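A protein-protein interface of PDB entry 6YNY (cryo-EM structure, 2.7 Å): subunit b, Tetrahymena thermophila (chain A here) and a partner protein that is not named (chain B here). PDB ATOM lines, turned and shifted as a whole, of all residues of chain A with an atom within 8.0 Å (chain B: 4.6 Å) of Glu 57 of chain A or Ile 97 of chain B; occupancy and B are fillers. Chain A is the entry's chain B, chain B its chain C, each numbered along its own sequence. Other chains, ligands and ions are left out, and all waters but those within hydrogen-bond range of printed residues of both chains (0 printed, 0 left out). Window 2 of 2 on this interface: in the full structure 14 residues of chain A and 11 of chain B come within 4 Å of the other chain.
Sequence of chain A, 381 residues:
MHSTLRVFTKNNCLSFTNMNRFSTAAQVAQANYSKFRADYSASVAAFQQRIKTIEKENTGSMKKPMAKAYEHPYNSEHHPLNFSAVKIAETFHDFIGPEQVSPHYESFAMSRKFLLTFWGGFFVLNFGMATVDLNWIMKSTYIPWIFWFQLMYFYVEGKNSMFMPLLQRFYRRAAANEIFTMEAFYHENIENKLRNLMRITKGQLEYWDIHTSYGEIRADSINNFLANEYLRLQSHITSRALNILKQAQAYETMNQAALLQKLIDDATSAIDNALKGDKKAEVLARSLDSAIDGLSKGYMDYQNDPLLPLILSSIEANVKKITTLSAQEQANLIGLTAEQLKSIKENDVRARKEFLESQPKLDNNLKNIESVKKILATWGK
Among the printed residues, merely in contact across the chains: Ile 54 of chain A with Leu 98 of chain B and Glu 57 of chain A with Ile 97 of chain B.
Of the 7 printed residues of chain B, 3 touch a printed residue of chain A.
Printed residues of chain B that touch a printed residue of chain A: Lys 95, Ile 97 and Leu 98.
Of the 14 printed residues of chain A, 4 touch a printed residue of chain B.
Printed residues of chain A that touch a printed residue of chain B: Arg 50, Ile 54, Glu 57 and Trp 208.
Hydrophobic or aromatic side chains of chain A within 4 Å of the printed part of chain B: Ile 54 and Trp 208.
O of Tyr 92 of chain B lies within hydrogen-bond range of N of Ile 97 of chain B (3.2 Å).
O of Asn 93 of chain B is in hydrogen-bond range of N of Leu 98 of chain B, at 2.8 Å.
The backbone carbonyl oxygen (O) of Lys 95 of chain B sits at hydrogen-bond distance from the indole nitrogen (NE1) of Trp 208 of chain A, at 3.0 Å.
The backbone carbonyl oxygen of Leu 98 of chain B is in hydrogen-bond range of the guanidinium group of Arg 50 of chain A, at 3.1 Å.
Of the printed residues of chain B, Arg 50 of chain A touches Leu 98.
Of the printed residues of chain B, Glu 57 of chain A touches Ile 97.
Tyr 92 of chain B touches none of the printed residues of chain A.
Of the printed residues of chain A, Ile 97 of chain B touches Glu 57.
Printed residues of chain A within 4 Å of Leu 98 of chain B: Arg 50 and Ile 54.
The nearest printed residue of chain A that does not touch Ile 97 of chain B is Thr 53 of chain A (4.4 Å).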
ATOM      1  N   GLN A  49     -15.949   1.878 -18.018  1.00  0.00           N
ATOM      2  CA  GLN A  49     -16.597   3.148 -17.722  1.00  0.00           C
ATOM      3  C   GLN A  49     -15.970   3.811 -16.507  1.00  0.00           C
ATOM      4  O   GLN A  49     -15.921   5.043 -16.425  1.00  0.00           O
ATOM      5  CB  GLN A  49     -18.094   2.939 -17.494  1.00  0.00           C
ATOM      6  CG  GLN A  49     -18.857   4.224 -17.231  1.00  0.00           C
ATOM      7  CD  GLN A  49     -18.735   5.212 -18.374  1.00  0.00           C
ATOM      8  OE1 GLN A  49     -18.877   4.850 -19.542  1.00  0.00           O
ATOM      9  NE2 GLN A  49     -18.460   6.468 -18.042  1.00  0.00           N
ATOM     10  N   ARG A  50     -15.490   3.013 -15.552  1.00  0.00           N
ATOM     11  CA  ARG A  50     -14.847   3.585 -14.376  1.00  0.00           C
ATOM     12  C   ARG A  50     -13.592   4.352 -14.768  1.00  0.00           C
ATOM     13  O   ARG A  50     -13.281   5.392 -14.177  1.00  0.00           O
ATOM     14  CB  ARG A  50     -14.513   2.480 -13.378  1.00  0.00           C
ATOM     15  CG  ARG A  50     -14.222   2.990 -11.986  1.00  0.00           C
ATOM     16  CD  ARG A  50     -14.159   1.855 -10.979  1.00  0.00           C
ATOM     17  NE  ARG A  50     -12.955   1.047 -11.133  1.00  0.00           N
ATOM     18  CZ  ARG A  50     -12.631   0.036 -10.333  1.00  0.00           C
ATOM     19  NH1 ARG A  50     -13.423  -0.293  -9.322  1.00  0.00           N
ATOM     20  NH2 ARG A  50     -11.514  -0.645 -10.542  1.00  0.00           N
ATOM     21  N   ILE A  51     -12.859   3.855 -15.765  1.00  0.00           N
ATOM     22  CA  ILE A  51     -11.677   4.564 -16.240  1.00  0.00           C
ATOM     23  C   ILE A  51     -12.069   5.919 -16.808  1.00  0.00           C
ATOM     24  O   ILE A  51     -11.298   6.883 -16.728  1.00  0.00           O
ATOM     25  CB  ILE A  51     -10.918   3.708 -17.271  1.00  0.00           C
ATOM     26  CG1 ILE A  51     -10.003   2.713 -16.557  1.00  0.00           C
ATOM     27  CG2 ILE A  51     -10.100   4.582 -18.208  1.00  0.00           C
ATOM     28  CD1 ILE A  51     -10.740   1.734 -15.677  1.00  0.00           C
ATOM     29  N   LYS A  52     -13.265   6.019 -17.390  1.00  0.00           N
ATOM     30  CA  LYS A  52     -13.726   7.303 -17.906  1.00  0.00           C
ATOM     31  C   LYS A  52     -13.814   8.335 -16.792  1.00  0.00           C
ATOM     32  O   LYS A  52     -13.437   9.497 -16.980  1.00  0.00           O
ATOM     33  CB  LYS A  52     -15.082   7.143 -18.592  1.00  0.00           C
ATOM     34  CG  LYS A  52     -15.110   6.098 -19.692  1.00  0.00           C
ATOM     35  CD  LYS A  52     -14.140   6.439 -20.808  1.00  0.00           C
ATOM     36  CE  LYS A  52     -14.208   5.421 -21.931  1.00  0.00           C
ATOM     37  NZ  LYS A  52     -13.254   5.743 -23.028  1.00  0.00           N
ATOM     38  N   THR A  53     -14.303   7.928 -15.620  1.00  0.00           N
ATOM     39  CA  THR A  53     -14.417   8.862 -14.507  1.00  0.00           C
ATOM     40  C   THR A  53     -13.044   9.366 -14.084  1.00  0.00           C
ATOM     41  O   THR A  53     -12.849  10.568 -13.869  1.00  0.00           O
ATOM     42  CB  THR A  53     -15.121   8.191 -13.328  1.00  0.00           C
ATOM     43  OG1 THR A  53     -14.329   7.095 -12.860  1.00  0.00           O
ATOM     44  CG2 THR A  53     -16.487   7.680 -13.740  1.00  0.00           C
ATOM     45  N   ILE A  54     -12.076   8.457 -13.964  1.00  0.00           N
ATOM     46  CA  ILE A  54     -10.733   8.855 -13.552  1.00  0.00           C
ATOM     47  C   ILE A  54     -10.188   9.925 -14.485  1.00  0.00           C
ATOM     48  O   ILE A  54      -9.552  10.890 -14.045  1.00  0.00           O
ATOM     49  CB  ILE A  54      -9.807   7.628 -13.499  1.00  0.00           C
ATOM     50  CG1 ILE A  54     -10.257   6.679 -12.388  1.00  0.00           C
ATOM     51  CG2 ILE A  54      -8.363   8.067 -13.301  1.00  0.00           C
ATOM     52  CD1 ILE A  54      -9.509   5.365 -12.359  1.00  0.00           C
ATOM     53  N   GLU A  55     -10.423   9.771 -15.788  1.00  0.00           N
ATOM     54  CA  GLU A  55      -9.966  10.777 -16.739  1.00  0.00           C
ATOM     55  C   GLU A  55     -10.648  12.112 -16.483  1.00  0.00           C
ATOM     56  O   GLU A  55      -9.994  13.162 -16.449  1.00  0.00           O
ATOM     57  CB  GLU A  55     -10.231  10.299 -18.164  1.00  0.00           C
ATOM     58  CG  GLU A  55      -9.489   9.026 -18.527  1.00  0.00           C
ATOM     59  CD  GLU A  55      -9.843   8.520 -19.911  1.00  0.00           C
ATOM     60  OE1 GLU A  55     -10.744   9.105 -20.548  1.00  0.00           O
ATOM     61  OE2 GLU A  55      -9.221   7.536 -20.363  1.00  0.00           O
ATOM     62  N   LYS A  56     -11.968  12.092 -16.295  1.00  0.00           N
ATOM     63  CA  LYS A  56     -12.688  13.329 -16.016  1.00  0.00           C
ATOM     64  C   LYS A  56     -12.219  13.948 -14.708  1.00  0.00           C
ATOM     65  O   LYS A  56     -12.104  15.174 -14.595  1.00  0.00           O
ATOM     66  CB  LYS A  56     -14.191  13.060 -15.977  1.00  0.00           C
ATOM     67  CG  LYS A  56     -14.733  12.463 -17.264  1.00  0.00           C
ATOM     68  CD  LYS A  56     -16.208  12.113 -17.157  1.00  0.00           C
ATOM     69  CE  LYS A  56     -17.075  13.360 -17.066  1.00  0.00           C
ATOM     70  NZ  LYS A  56     -18.530  13.039 -17.061  1.00  0.00           N
ATOM     71  N   GLU A  57     -11.943  13.112 -13.705  1.00  0.00           N
ATOM     72  CA  GLU A  57     -11.473  13.619 -12.423  1.00  0.00           C
ATOM     73  C   GLU A  57     -10.084  14.227 -12.539  1.00  0.00           C
ATOM     74  O   GLU A  57      -9.773  15.201 -11.844  1.00  0.00           O
ATOM     75  CB  GLU A  57     -11.480  12.497 -11.388  1.00  0.00           C
ATOM     76  CG  GLU A  57     -12.868  11.999 -11.032  1.00  0.00           C
ATOM     77  CD  GLU A  57     -13.693  13.041 -10.302  1.00  0.00           C
ATOM     78  OE1 GLU A  57     -13.117  14.061  -9.869  1.00  0.00           O
ATOM     79  OE2 GLU A  57     -14.917  12.841 -10.164  1.00  0.00           O
ATOM     80  N   ASN A  58      -9.238  13.671 -13.408  1.00  0.00           N
ATOM     81  CA  ASN A  58      -7.887  14.190 -13.571  1.00  0.00           C
ATOM     82  C   ASN A  58      -7.885  15.618 -14.096  1.00  0.00           C
ATOM     83  O   ASN A  58      -6.909  16.345 -13.881  1.00  0.00           O
ATOM     84  CB  ASN A  58      -7.094  13.285 -14.513  1.00  0.00           C
ATOM     85  CG  ASN A  58      -5.620  13.628 -14.545  1.00  0.00           C
ATOM     86  OD1 ASN A  58      -5.183  14.471 -15.329  1.00  0.00           O
ATOM     87  ND2 ASN A  58      -4.842  12.973 -13.690  1.00  0.00           N
ATOM     88  N   THR A  59      -8.955  16.035 -14.773  1.00  0.00           N
ATOM     89  CA  THR A  59      -9.055  17.386 -15.313  1.00  0.00           C
ATOM     90  C   THR A  59      -9.301  18.439 -14.241  1.00  0.00           C
ATOM     91  O   THR A  59      -9.337  19.630 -14.570  1.00  0.00           O
ATOM     92  CB  THR A  59     -10.180  17.453 -16.349  1.00  0.00           C
ATOM     93  OG1 THR A  59     -11.445  17.311 -15.691  1.00  0.00           O
ATOM     94  CG2 THR A  59     -10.029  16.344 -17.381  1.00  0.00           C
ATOM     95  N   GLY A  60      -9.477  18.040 -12.984  1.00  0.00           N
ATOM     96  CA  GLY A  60      -9.766  18.977 -11.917  1.00  0.00           C
ATOM     97  C   GLY A  60      -8.769  20.112 -11.797  1.00  0.00           C
ATOM     98  O   GLY A  60      -7.565  19.917 -11.989  1.00  0.00           O
ATOM     99  N   SER A  61      -9.265  21.305 -11.475  1.00  0.00           N
ATOM    100  CA  SER A  61      -8.448  22.493 -11.267  1.00  0.00           C
ATOM    101  C   SER A  61      -8.822  23.115  -9.926  1.00  0.00           C
ATOM    102  O   SER A  61      -9.696  22.618  -9.209  1.00  0.00           O
ATOM    103  CB  SER A  61      -8.624  23.499 -12.411  1.00  0.00           C
ATOM    104  OG  SER A  61      -9.978  23.894 -12.542  1.00  0.00           O
ATOM    105  N   TRP A 208     -24.913   1.820   1.825  1.00  0.00           N
ATOM    106  CA  TRP A 208     -24.193   2.077   0.586  1.00  0.00           C
ATOM    107  C   TRP A 208     -23.585   0.807   0.013  1.00  0.00           C
ATOM    108  O   TRP A 208     -23.498   0.665  -1.211  1.00  0.00           O
ATOM    109  CB  TRP A 208     -23.110   3.124   0.826  1.00  0.00           C
ATOM    110  CG  TRP A 208     -22.266   3.416  -0.367  1.00  0.00           C
ATOM    111  CD1 TRP A 208     -20.952   3.114  -0.527  1.00  0.00           C
ATOM    112  CD2 TRP A 208     -22.679   4.068  -1.570  1.00  0.00           C
ATOM    113  NE1 TRP A 208     -20.515   3.539  -1.754  1.00  0.00           N
ATOM    114  CE2 TRP A 208     -21.559   4.129  -2.415  1.00  0.00           C
ATOM    115  CE3 TRP A 208     -23.886   4.607  -2.016  1.00  0.00           C
ATOM    116  CZ2 TRP A 208     -21.609   4.704  -3.678  1.00  0.00           C
ATOM    117  CZ3 TRP A 208     -23.934   5.177  -3.265  1.00  0.00           C
ATOM    118  CH2 TRP A 208     -22.804   5.223  -4.083  1.00  0.00           C
ATOM    119  N   TYR B  92     -13.787   9.098  -0.132  1.00  0.00           N
ATOM    120  CA  TYR B  92     -14.749   9.465  -1.164  1.00  0.00           C
ATOM    121  C   TYR B  92     -14.399   8.822  -2.498  1.00  0.00           C
ATOM    122  O   TYR B  92     -15.244   8.179  -3.129  1.00  0.00           O
ATOM    123  CB  TYR B  92     -14.810  10.983  -1.311  1.00  0.00           C
ATOM    124  CG  TYR B  92     -15.427  11.719  -0.147  1.00  0.00           C
ATOM    125  CD1 TYR B  92     -15.800  11.057   1.009  1.00  0.00           C
ATOM    126  CD2 TYR B  92     -15.648  13.083  -0.216  1.00  0.00           C
ATOM    127  CE1 TYR B  92     -16.364  11.734   2.063  1.00  0.00           C
ATOM    128  CE2 TYR B  92     -16.211  13.765   0.832  1.00  0.00           C
ATOM    129  CZ  TYR B  92     -16.568  13.088   1.967  1.00  0.00           C
ATOM    130  OH  TYR B  92     -17.133  13.773   3.012  1.00  0.00           O
ATOM    131  N   ASN B  93     -13.156   8.994  -2.947  1.00  0.00           N
ATOM    132  CA  ASN B  93     -12.771   8.490  -4.259  1.00  0.00           C
ATOM    133  C   ASN B  93     -12.918   6.980  -4.347  1.00  0.00           C
ATOM    134  O   ASN B  93     -13.275   6.451  -5.405  1.00  0.00           O
ATOM    135  CB  ASN B  93     -11.333   8.894  -4.572  1.00  0.00           C
ATOM    136  CG  ASN B  93     -11.115  10.387  -4.487  1.00  0.00           C
ATOM    137  OD1 ASN B  93     -12.019  11.175  -4.760  1.00  0.00           O
ATOM    138  ND2 ASN B  93      -9.910  10.785  -4.104  1.00  0.00           N
ATOM    139  N   LYS B  95     -14.970   4.840  -2.451  1.00  0.00           N
ATOM    140  CA  LYS B  95     -16.303   4.295  -2.234  1.00  0.00           C
ATOM    141  C   LYS B  95     -17.389   5.020  -3.013  1.00  0.00           C
ATOM    142  O   LYS B  95     -18.291   4.371  -3.549  1.00  0.00           O
ATOM    143  CB  LYS B  95     -16.641   4.329  -0.745  1.00  0.00           C
ATOM    144  CG  LYS B  95     -15.624   3.616   0.111  1.00  0.00           C
ATOM    145  CD  LYS B  95     -16.093   3.478   1.537  1.00  0.00           C
ATOM    146  CE  LYS B  95     -17.115   2.367   1.688  1.00  0.00           C
ATOM    147  NZ  LYS B  95     -16.536   1.035   1.376  1.00  0.00           N
ATOM    148  N   LEU B  96     -17.333   6.347  -3.089  1.00  0.00           N
ATOM    149  CA  LEU B  96     -18.380   7.088  -3.780  1.00  0.00           C
ATOM    150  C   LEU B  96     -18.130   7.171  -5.277  1.00  0.00           C
ATOM    151  O   LEU B  96     -19.080   7.317  -6.052  1.00  0.00           O
ATOM    152  CB  LEU B  96     -18.500   8.497  -3.205  1.00  0.00           C
ATOM    153  CG  LEU B  96     -18.641   8.601  -1.691  1.00  0.00           C
ATOM    154  CD1 LEU B  96     -18.816  10.047  -1.302  1.00  0.00           C
ATOM    155  CD2 LEU B  96     -19.795   7.771  -1.194  1.00  0.00           C
ATOM    156  N   ILE B  97     -16.873   7.083  -5.700  1.00  0.00           N
ATOM    157  CA  ILE B  97     -16.498   7.208  -7.104  1.00  0.00           C
ATOM    158  C   ILE B  97     -16.083   5.860  -7.686  1.00  0.00           C
ATOM    159  O   ILE B  97     -16.690   5.373  -8.642  1.00  0.00           O
ATOM    160  CB  ILE B  97     -15.384   8.262  -7.282  1.00  0.00           C
ATOM    161  CG1 ILE B  97     -15.853   9.603  -6.718  1.00  0.00           C
ATOM    162  CG2 ILE B  97     -15.000   8.388  -8.741  1.00  0.00           C
ATOM    163  CD1 ILE B  97     -14.835  10.697  -6.808  1.00  0.00           C
ATOM    164  N   LEU B  98     -15.050   5.244  -7.125  1.00  0.00           N
ATOM    165  CA  LEU B  98     -14.546   3.969  -7.614  1.00  0.00           C
ATOM    166  C   LEU B  98     -15.253   2.770  -6.999  1.00  0.00           C
ATOM    167  O   LEU B  98     -14.899   1.631  -7.321  1.00  0.00           O
ATOM    168  CB  LEU B  98     -13.044   3.862  -7.343  1.00  0.00           C
ATOM    169  CG  LEU B  98     -12.182   4.970  -7.947  1.00  0.00           C
ATOM    170  CD1 LEU B  98     -10.749   4.831  -7.481  1.00  0.00           C
ATOM    171  CD2 LEU B  98     -12.255   4.947  -9.459  1.00  0.00           C
ATOM    172  N   LYS B  99     -16.237   2.991  -6.136  1.00  0.00           N
ATOM    173  CA  LYS B  99     -16.921   1.899  -5.457  1.00  0.00           C
ATOM    174  C   LYS B  99     -15.928   0.979  -4.754  1.00  0.00           C
ATOM    175  O   LYS B  99     -15.488  -0.022  -5.318  1.00  0.00           O
ATOM    176  CB  LYS B  99     -17.768   1.099  -6.441  1.00  0.00           C
ATOM    177  CG  LYS B  99     -19.160   1.662  -6.662  1.00  0.00           C
ATOM    178  CD  LYS B  99     -19.126   3.051  -7.263  1.00  0.00           C
ATOM    179  CE  LYS B  99     -20.529   3.548  -7.550  1.00  0.00           C
ATOM    180  NZ  LYS B  99     -20.540   4.895  -8.165  1.00  0.00           N
